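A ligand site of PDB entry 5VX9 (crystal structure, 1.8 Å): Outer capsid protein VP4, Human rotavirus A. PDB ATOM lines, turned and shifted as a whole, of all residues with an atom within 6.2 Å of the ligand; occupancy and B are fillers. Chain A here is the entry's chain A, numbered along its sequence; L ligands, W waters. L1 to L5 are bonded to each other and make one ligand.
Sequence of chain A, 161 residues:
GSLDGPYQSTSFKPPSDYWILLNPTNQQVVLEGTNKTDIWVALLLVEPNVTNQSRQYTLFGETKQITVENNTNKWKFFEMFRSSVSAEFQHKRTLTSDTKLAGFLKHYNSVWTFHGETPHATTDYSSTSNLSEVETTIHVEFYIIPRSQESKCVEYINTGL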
ATOM      1  N   TRP A  19     -11.435  11.873   1.821  1.00  0.00           N
ATOM      2  CA  TRP A  19     -10.987  10.819   0.908  1.00  0.00           C
ATOM      3  C   TRP A  19     -10.170  11.397  -0.230  1.00  0.00           C
ATOM      4  O   TRP A  19     -10.537  12.430  -0.808  1.00  0.00           O
ATOM      5  CB  TRP A  19     -12.167  10.035   0.316  1.00  0.00           C
ATOM      6  CG  TRP A  19     -12.713   8.971   1.235  1.00  0.00           C
ATOM      7  CD1 TRP A  19     -13.805   9.058   2.040  1.00  0.00           C
ATOM      8  CD2 TRP A  19     -12.176   7.657   1.417  1.00  0.00           C
ATOM      9  NE1 TRP A  19     -13.989   7.879   2.731  1.00  0.00           N
ATOM     10  CE2 TRP A  19     -12.995   7.004   2.371  1.00  0.00           C
ATOM     11  CE3 TRP A  19     -11.058   6.980   0.911  1.00  0.00           C
ATOM     12  CZ2 TRP A  19     -12.738   5.705   2.799  1.00  0.00           C
ATOM     13  CZ3 TRP A  19     -10.824   5.675   1.339  1.00  0.00           C
ATOM     14  CH2 TRP A  19     -11.648   5.056   2.278  1.00  0.00           C
ATOM     15  N   LEU A 105      -7.800   7.415   2.878  1.00  0.00           N
ATOM     16  CA  LEU A 105      -8.384   8.284   3.891  1.00  0.00           C
ATOM     17  C   LEU A 105      -7.634   8.209   5.211  1.00  0.00           C
ATOM     18  O   LEU A 105      -7.274   7.125   5.653  1.00  0.00           O
ATOM     19  CB  LEU A 105      -9.848   7.908   4.133  1.00  0.00           C
ATOM     20  CG  LEU A 105     -10.509   8.543   5.357  1.00  0.00           C
ATOM     21  CD1 LEU A 105     -10.726  10.007   5.094  1.00  0.00           C
ATOM     22  CD2 LEU A 105     -11.820   7.850   5.714  1.00  0.00           C
ATOM     23  N   HIS A 107      -8.452   8.859   9.082  1.00  0.00           N
ATOM     24  CA  HIS A 107      -9.566   9.123   9.997  1.00  0.00           C
ATOM     25  C   HIS A 107      -9.368   8.445  11.353  1.00  0.00           C
ATOM     26  O   HIS A 107      -9.068   7.244  11.403  1.00  0.00           O
ATOM     27  CB  HIS A 107     -10.904   8.670   9.400  1.00  0.00           C
ATOM     28  CG  HIS A 107     -12.060   8.866  10.337  1.00  0.00           C
ATOM     29  ND1 HIS A 107     -12.562  10.098  10.666  1.00  0.00           N
ATOM     30  CD2 HIS A 107     -12.770   7.970  11.068  1.00  0.00           C
ATOM     31  CE1 HIS A 107     -13.552   9.963  11.524  1.00  0.00           C
ATOM     32  NE2 HIS A 107     -13.695   8.680  11.800  1.00  0.00           N
ATOM     33  N   TYR A 108      -9.556   9.215  12.420  1.00  0.00           N
ATOM     34  CA  TYR A 108      -9.547   8.722  13.801  1.00  0.00           C
ATOM     35  C   TYR A 108      -8.173   8.160  14.147  1.00  0.00           C
ATOM     36  O   TYR A 108      -7.243   8.925  14.396  1.00  0.00           O
ATOM     37  CB  TYR A 108     -10.661   7.692  14.011  1.00  0.00           C
ATOM     38  CG  TYR A 108     -10.975   7.374  15.473  1.00  0.00           C
ATOM     39  CD1 TYR A 108     -11.486   8.352  16.332  1.00  0.00           C
ATOM     40  CD2 TYR A 108     -10.769   6.103  15.976  1.00  0.00           C
ATOM     41  CE1 TYR A 108     -11.765   8.053  17.658  1.00  0.00           C
ATOM     42  CE2 TYR A 108     -11.055   5.797  17.298  1.00  0.00           C
ATOM     43  CZ  TYR A 108     -11.550   6.775  18.130  1.00  0.00           C
ATOM     44  OH  TYR A 108     -11.826   6.464  19.443  1.00  0.00           O
ATOM     45  N   ASN A 109      -8.027   6.841  14.165  1.00  0.00           N
ATOM     46  CA  ASN A 109      -6.740   6.250  14.482  1.00  0.00           C
ATOM     47  C   ASN A 109      -6.169   5.413  13.328  1.00  0.00           C
ATOM     48  O   ASN A 109      -5.310   4.581  13.553  1.00  0.00           O
ATOM     49  CB  ASN A 109      -6.843   5.377  15.729  1.00  0.00           C
ATOM     50  CG  ASN A 109      -7.751   4.166  15.514  1.00  0.00           C
ATOM     51  OD1 ASN A 109      -8.500   4.111  14.539  1.00  0.00           O
ATOM     52  ND2 ASN A 109      -7.687   3.199  16.430  1.00  0.00           N
ATOM     53  N   SER A 110      -6.657   5.629  12.112  1.00  0.00           N
ATOM     54  CA  SER A 110      -6.360   4.691  11.036  1.00  0.00           C
ATOM     55  C   SER A 110      -6.246   5.340   9.664  1.00  0.00           C
ATOM     56  O   SER A 110      -6.782   6.427   9.428  1.00  0.00           O
ATOM     57  CB  SER A 110      -7.450   3.625  10.940  1.00  0.00           C
ATOM     58  OG  SER A 110      -7.521   2.808  12.103  1.00  0.00           O
ATOM     59  N   TRP A 112      -7.422   4.392   5.856  1.00  0.00           N
ATOM     60  CA  TRP A 112      -8.406   3.537   5.191  1.00  0.00           C
ATOM     61  C   TRP A 112      -8.155   3.431   3.692  1.00  0.00           C
ATOM     62  O   TRP A 112      -7.754   4.400   3.057  1.00  0.00           O
ATOM     63  CB  TRP A 112      -9.820   4.077   5.429  1.00  0.00           C
ATOM     64  CG  TRP A 112     -10.225   4.027   6.875  1.00  0.00           C
ATOM     65  CD1 TRP A 112      -9.862   4.895   7.872  1.00  0.00           C
ATOM     66  CD2 TRP A 112     -11.053   3.036   7.481  1.00  0.00           C
ATOM     67  NE1 TRP A 112     -10.436   4.503   9.061  1.00  0.00           N
ATOM     68  CE2 TRP A 112     -11.162   3.355   8.856  1.00  0.00           C
ATOM     69  CE3 TRP A 112     -11.720   1.891   7.003  1.00  0.00           C
ATOM     70  CZ2 TRP A 112     -11.905   2.581   9.746  1.00  0.00           C
ATOM     71  CZ3 TRP A 112     -12.456   1.122   7.896  1.00  0.00           C
ATOM     72  CH2 TRP A 112     -12.539   1.474   9.256  1.00  0.00           C
ATOM     73  N   THR A 122     -15.331  -2.493  -0.564  1.00  0.00           N
ATOM     74  CA  THR A 122     -15.631  -1.968   0.764  1.00  0.00           C
ATOM     75  C   THR A 122     -14.355  -1.423   1.392  1.00  0.00           C
ATOM     76  O   THR A 122     -13.282  -1.559   0.832  1.00  0.00           O
ATOM     77  CB  THR A 122     -16.238  -3.040   1.679  1.00  0.00           C
ATOM     78  OG1 THR A 122     -15.324  -4.138   1.785  1.00  0.00           O
ATOM     79  CG2 THR A 122     -17.548  -3.545   1.125  1.00  0.00           C
ATOM     80  N   THR A 123     -14.470  -0.817   2.580  1.00  0.00           N
ATOM     81  CA  THR A 123     -13.341  -0.156   3.211  1.00  0.00           C
ATOM     82  C   THR A 123     -12.707  -1.021   4.307  1.00  0.00           C
ATOM     83  O   THR A 123     -13.401  -1.809   4.959  1.00  0.00           O
ATOM     84  CB  THR A 123     -13.771   1.185   3.847  1.00  0.00           C
ATOM     85  OG1 THR A 123     -14.821   0.933   4.774  1.00  0.00           O
ATOM     86  CG2 THR A 123     -14.256   2.152   2.789  1.00  0.00           C
ATOM     87  N   ASP A 124     -11.411  -0.872   4.519  1.00  0.00           N
ATOM     88  CA  ASP A 124     -10.745  -1.522   5.679  1.00  0.00           C
ATOM     89  C   ASP A 124      -9.556  -0.665   6.082  1.00  0.00           C
ATOM     90  O   ASP A 124      -9.158   0.234   5.353  1.00  0.00           O
ATOM     91  CB  ASP A 124     -10.321  -2.964   5.335  1.00  0.00           C
ATOM     92  CG  ASP A 124      -9.993  -3.800   6.583  1.00  0.00           C
ATOM     93  OD1 ASP A 124     -10.362  -3.425   7.727  1.00  0.00           O
ATOM     94  OD2 ASP A 124      -9.354  -4.870   6.401  1.00  0.00           O
ATOM     95  N   TYR A 125      -8.988  -0.924   7.265  1.00  0.00           N
ATOM     96  CA  TYR A 125      -8.072   0.040   7.874  1.00  0.00           C
ATOM     97  C   TYR A 125      -6.762  -0.564   8.340  1.00  0.00           C
ATOM     98  O   TYR A 125      -6.671  -1.775   8.548  1.00  0.00           O
ATOM     99  CB  TYR A 125      -8.754   0.745   9.063  1.00  0.00           C
ATOM    100  CG  TYR A 125      -9.026  -0.159  10.258  1.00  0.00           C
ATOM    101  CD1 TYR A 125     -10.230  -0.860  10.369  1.00  0.00           C
ATOM    102  CD2 TYR A 125      -8.094  -0.302  11.280  1.00  0.00           C
ATOM    103  CE1 TYR A 125     -10.482  -1.679  11.461  1.00  0.00           C
ATOM    104  CE2 TYR A 125      -8.340  -1.129  12.373  1.00  0.00           C
ATOM    105  CZ  TYR A 125      -9.522  -1.815  12.452  1.00  0.00           C
ATOM    106  OH  TYR A 125      -9.776  -2.624  13.534  1.00  0.00           O
ATOM    107  N   SER A 127      -4.247   0.611  11.602  1.00  0.00           N
ATOM    108  CA  SER A 127      -4.212   1.600  12.687  1.00  0.00           C
ATOM    109  C   SER A 127      -2.804   2.160  12.897  1.00  0.00           C
ATOM    110  O   SER A 127      -1.800   1.566  12.498  1.00  0.00           O
ATOM    111  CB  SER A 127      -4.747   1.006  13.986  1.00  0.00           C
ATOM    112  OG  SER A 127      -4.000  -0.127  14.380  1.00  0.00           O
ATOM    113  N   ARG A 147     -15.435  13.087   4.168  1.00  0.00           N
ATOM    114  CA  ARG A 147     -15.929  11.842   4.712  1.00  0.00           C
ATOM    115  C   ARG A 147     -17.453  11.869   4.894  1.00  0.00           C
ATOM    116  O   ARG A 147     -18.115  10.839   4.830  1.00  0.00           O
ATOM    117  CB  ARG A 147     -15.223  11.520   6.032  1.00  0.00           C
ATOM    118  CG  ARG A 147     -15.523  10.158   6.591  1.00  0.00           C
ATOM    119  CD  ARG A 147     -14.903   9.976   7.966  1.00  0.00           C
ATOM    120  NE  ARG A 147     -15.212   8.658   8.531  1.00  0.00           N
ATOM    121  CZ  ARG A 147     -16.178   8.417   9.417  1.00  0.00           C
ATOM    122  NH1 ARG A 147     -16.938   9.411   9.863  1.00  0.00           N
ATOM    123  NH2 ARG A 147     -16.380   7.186   9.847  1.00  0.00           N
ATOM    124  N   GLU A 150     -18.857  10.111   2.025  1.00  0.00           N
ATOM    125  CA  GLU A 150     -18.194   8.852   1.720  1.00  0.00           C
ATOM    126  C   GLU A 150     -19.024   7.985   0.782  1.00  0.00           C
ATOM    127  O   GLU A 150     -18.472   7.266  -0.043  1.00  0.00           O
ATOM    128  CB  GLU A 150     -17.864   8.068   2.991  1.00  0.00           C
ATOM    129  CG  GLU A 150     -17.320   6.669   2.694  1.00  0.00           C
ATOM    130  CD  GLU A 150     -16.560   6.065   3.847  1.00  0.00           C
ATOM    131  OE1 GLU A 150     -16.691   4.837   4.052  1.00  0.00           O
ATOM    132  OE2 GLU A 150     -15.827   6.794   4.537  1.00  0.00           O
ATOM    133  N   VAL A 154     -17.725   5.915  -2.449  1.00  0.00           N
ATOM    134  CA  VAL A 154     -17.953   4.478  -2.661  1.00  0.00           C
ATOM    135  C   VAL A 154     -18.597   4.230  -4.015  1.00  0.00           C
ATOM    136  O   VAL A 154     -18.232   3.299  -4.733  1.00  0.00           O
ATOM    137  CB  VAL A 154     -18.829   3.880  -1.539  1.00  0.00           C
ATOM    138  CG1 VAL A 154     -19.116   2.407  -1.794  1.00  0.00           C
ATOM    139  CG2 VAL A 154     -18.122   4.036  -0.193  1.00  0.00           C
HETATM  140  C1  LIG L   1     -11.020   1.116  17.394  1.00  0.00           C
HETATM  141  C2  LIG L   1     -12.374   1.311  16.714  1.00  0.00           C
HETATM  142  C3  LIG L   1     -12.193   1.947  15.342  1.00  0.00           C
HETATM  143  C4  LIG L   1     -11.200   1.061  14.562  1.00  0.00           C
HETATM  144  C5  LIG L   1     -10.835   1.623  13.189  1.00  0.00           C
HETATM  145  C6  LIG L   1     -10.112   0.321  16.492  1.00  0.00           C
HETATM  146  O1  LIG L   1      -8.826   0.196  17.095  1.00  0.00           O
HETATM  147  O2  LIG L   1     -11.188   0.381  18.637  1.00  0.00           O
HETATM  148  O3  LIG L   1     -13.221   2.145  17.506  1.00  0.00           O
HETATM  149  O4  LIG L   1     -13.482   2.003  14.666  1.00  0.00           O
HETATM  150  O5  LIG L   1      -9.961   1.005  15.251  1.00  0.00           O
HETATM  151  O6  LIG L   1     -10.444   3.003  13.318  1.00  0.00           O
HETATM  152  C1  LG2 L   2     -13.699   3.218  13.970  1.00  0.00           C
HETATM  153  C2  LG2 L   2     -14.774   2.988  12.902  1.00  0.00           C
HETATM  154  C3  LG2 L   2     -14.903   4.248  12.064  1.00  0.00           C
HETATM  155  C4  LG2 L   2     -15.182   5.442  12.977  1.00  0.00           C
HETATM  156  C5  LG2 L   2     -14.144   5.510  14.112  1.00  0.00           C
HETATM  157  C6  LG2 L   2     -14.467   6.662  15.086  1.00  0.00           C
HETATM  158  O1  LG2 L   2     -14.381   1.871  12.074  1.00  0.00           O
HETATM  159  O2  LG2 L   2     -16.017   4.111  11.179  1.00  0.00           O
HETATM  160  O3  LG2 L   2     -16.498   5.282  13.514  1.00  0.00           O
HETATM  161  O4  LG2 L   2     -14.117   4.268  14.860  1.00  0.00           O
HETATM  162  O5  LG2 L   2     -14.651   7.875  14.358  1.00  0.00           O
HETATM  163  C1  LG3 L   3     -15.701   3.626   9.889  1.00  0.00           C
HETATM  164  C2  LG3 L   3     -17.022   3.367   9.191  1.00  0.00           C
HETATM  165  C3  LG3 L   3     -16.781   2.980   7.752  1.00  0.00           C
HETATM  166  C4  LG3 L   3     -15.868   3.996   7.086  1.00  0.00           C
HETATM  167  C5  LG3 L   3     -14.625   4.240   7.915  1.00  0.00           C
HETATM  168  C6  LG3 L   3     -13.740   5.349   7.293  1.00  0.00           C
HETATM  169  C7  LG3 L   3     -18.745   2.453  10.709  1.00  0.00           C
HETATM  170  C8  LG3 L   3     -19.342   1.184  11.317  1.00  0.00           C
HETATM  171  N1  LG3 L   3     -17.713   2.257   9.867  1.00  0.00           N
HETATM  172  O1  LG3 L   3     -18.037   3.035   7.045  1.00  0.00           O
HETATM  173  O2  LG3 L   3     -15.504   3.447   5.800  1.00  0.00           O
HETATM  174  O3  LG3 L   3     -15.009   4.675   9.222  1.00  0.00           O
HETATM  175  O4  LG3 L   3     -14.544   6.476   6.908  1.00  0.00           O
HETATM  176  O5  LG3 L   3     -19.218   3.553  10.974  1.00  0.00           O
HETATM  177  C1  LG4 L   4     -18.791   1.819   6.912  1.00  0.00           C
HETATM  178  C2  LG4 L   4     -20.226   2.168   6.501  1.00  0.00           C
HETATM  179  C3  LG4 L   4     -21.021   0.882   6.314  1.00  0.00           C
HETATM  180  C4  LG4 L   4     -20.336  -0.025   5.298  1.00  0.00           C
HETATM  181  C5  LG4 L   4     -18.872  -0.226   5.722  1.00  0.00           C
HETATM  182  C6  LG4 L   4     -18.166  -1.117   4.696  1.00  0.00           C
HETATM  183  O1  LG4 L   4     -20.841   2.955   7.560  1.00  0.00           O
HETATM  184  O2  LG4 L   4     -22.341   1.200   5.820  1.00  0.00           O
HETATM  185  O3  LG4 L   4     -20.393   0.612   3.998  1.00  0.00           O
HETATM  186  O4  LG4 L   4     -18.195   1.055   5.830  1.00  0.00           O
HETATM  187  O5  LG4 L   4     -16.760  -1.060   4.917  1.00  0.00           O
HETATM  188  C1  LG5 L   5     -21.631   4.050   7.073  1.00  0.00           C
HETATM  189  C2  LG5 L   5     -22.547   4.549   8.199  1.00  0.00           C
HETATM  190  C3  LG5 L   5     -21.733   5.151   9.331  1.00  0.00           C
HETATM  191  C4  LG5 L   5     -20.838   6.261   8.811  1.00  0.00           C
HETATM  192  C5  LG5 L   5     -19.971   5.686   7.682  1.00  0.00           C
HETATM  193  C6  LG5 L   5     -19.076   6.806   7.122  1.00  0.00           C
HETATM  194  O1  LG5 L   5     -23.331   3.448   8.708  1.00  0.00           O
HETATM  195  O2  LG5 L   5     -22.627   5.710  10.313  1.00  0.00           O
HETATM  196  O3  LG5 L   5     -21.643   7.370   8.333  1.00  0.00           O
HETATM  197  O4  LG5 L   5     -20.794   5.157   6.608  1.00  0.00           O
HETATM  198  O   HOH W   1     -18.314   2.791   3.261  1.00  0.00           O
HETATM  199  O   HOH W   2     -22.574   0.860   9.639  1.00  0.00           O
HETATM  200  O   HOH W   3     -18.281   6.022  11.555  1.00  0.00           O
HETATM  201  O   HOH W   4     -14.968  -1.384   7.264  1.00  0.00           O
HETATM  202  O   HOH W   5     -23.011   2.567   3.620  1.00  0.00           O
HETATM  203  O   HOH W   6     -14.397  -1.312  10.968  1.00  0.00           O
HETATM  204  O   HOH W   7     -21.168   3.753  12.845  1.00  0.00           O
HETATM  205  O   HOH W   8     -20.844  10.070   8.618  1.00  0.00           O
HETATM  206  O   HOH W   9     -10.937   5.215  11.741  1.00  0.00           O
HETATM  207  O   HOH W  10     -16.691  -0.464   9.286  1.00  0.00           O
HETATM  208  O   HOH W  11     -21.411   6.269   4.082  1.00  0.00           O
HETATM  209  O   HOH W  12     -15.405   4.011  17.562  1.00  0.00           O
HETATM  210  O   HOH W  13      -6.933  -2.180  15.892  1.00  0.00           O
HETATM  211  O   HOH W  14     -17.572   3.417  15.300  1.00  0.00           O
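OD1 of Asn 109 sits at hydrogen-bond distance from OG of Ser 110 (2.9 Å). O of Leu 105 sits at hydrogen-bond distance from N of Trp 112, 2.7 Å away. The side-chain carboxylate (OE2) of Glu 150 is in hydrogen-bond range of the indole nitrogen (NE1) of Trp 19.
Water W3 bridges O5 of LG3 L3 and NH2 of Arg 147. Water W9 lies within hydrogen-bond range of O6 of LIG L1 (2.8 Å), O of His 107 (2.8 Å) and NE1 of Trp 112 (2.8 Å). Water W4 lies within hydrogen-bond range of O of Thr 123 and O5 of LG4 L4. Water W1 lies within hydrogen-bond range of the side-chain carboxylate of Glu 150 (2.7 Å) and an oxygen (O3) of LG4 L4 (3.1 Å).
O5 of LG2 L2 is in hydrogen-bond range of NE2 of His 107 (2.8 Å). An oxygen (O6) of LIG L1 sits at hydrogen-bond distance from the side-chain hydroxyl (OG) of Ser 110 (3.2 Å). The backbone carbonyl oxygen (O) of Thr 123 is in hydrogen-bond range of an oxygen (O5) of LG4 L4, at 3.4 Å. The side-chain carboxylate (OE1) of Glu 150 is in hydrogen-bond range of an oxygen (O2) of LG3 L3 (2.5 Å). An oxygen (O5) of LG4 L4 is in hydrogen-bond range of the side-chain hydroxyl (OG1) of Thr 123. The backbone NH of Thr 123 is in hydrogen-bond range of an oxygen (O5) of LG4 L4 (3.3 Å). The side-chain amide oxygen (OD1) of Asn 109 is in hydrogen-bond range of an oxygen (O6) of LIG L1 (2.5 Å). The guanidinium group of Arg 147 lies within hydrogen-bond range of an oxygen (O4) of LG3 L3, at 2.8 Å.
Leu 105 touches the ligand. Tyr 108 touches the ligand. CH2 of Trp 112 touches O1 of LG2 L2, at 3.4 Å. Thr 122 touches the ligand. CE1 of Tyr 125 touches C5 of LIG L1, at 3.7 Å. Hydrophobic or aromatic side chains within 4 Å of the ligand: Leu 105, His 107, Tyr 108, Trp 112 and Tyr 125. Within 4 Å of the ligand: Leu 105, His 107, Tyr 108, Asn 109, Ser 110, Trp 112, Thr 122, Thr 123, Tyr 125, Arg 147 and Glu 150. The nearest printed residue that does not touch the ligand is Trp 19 (4.4 Å).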
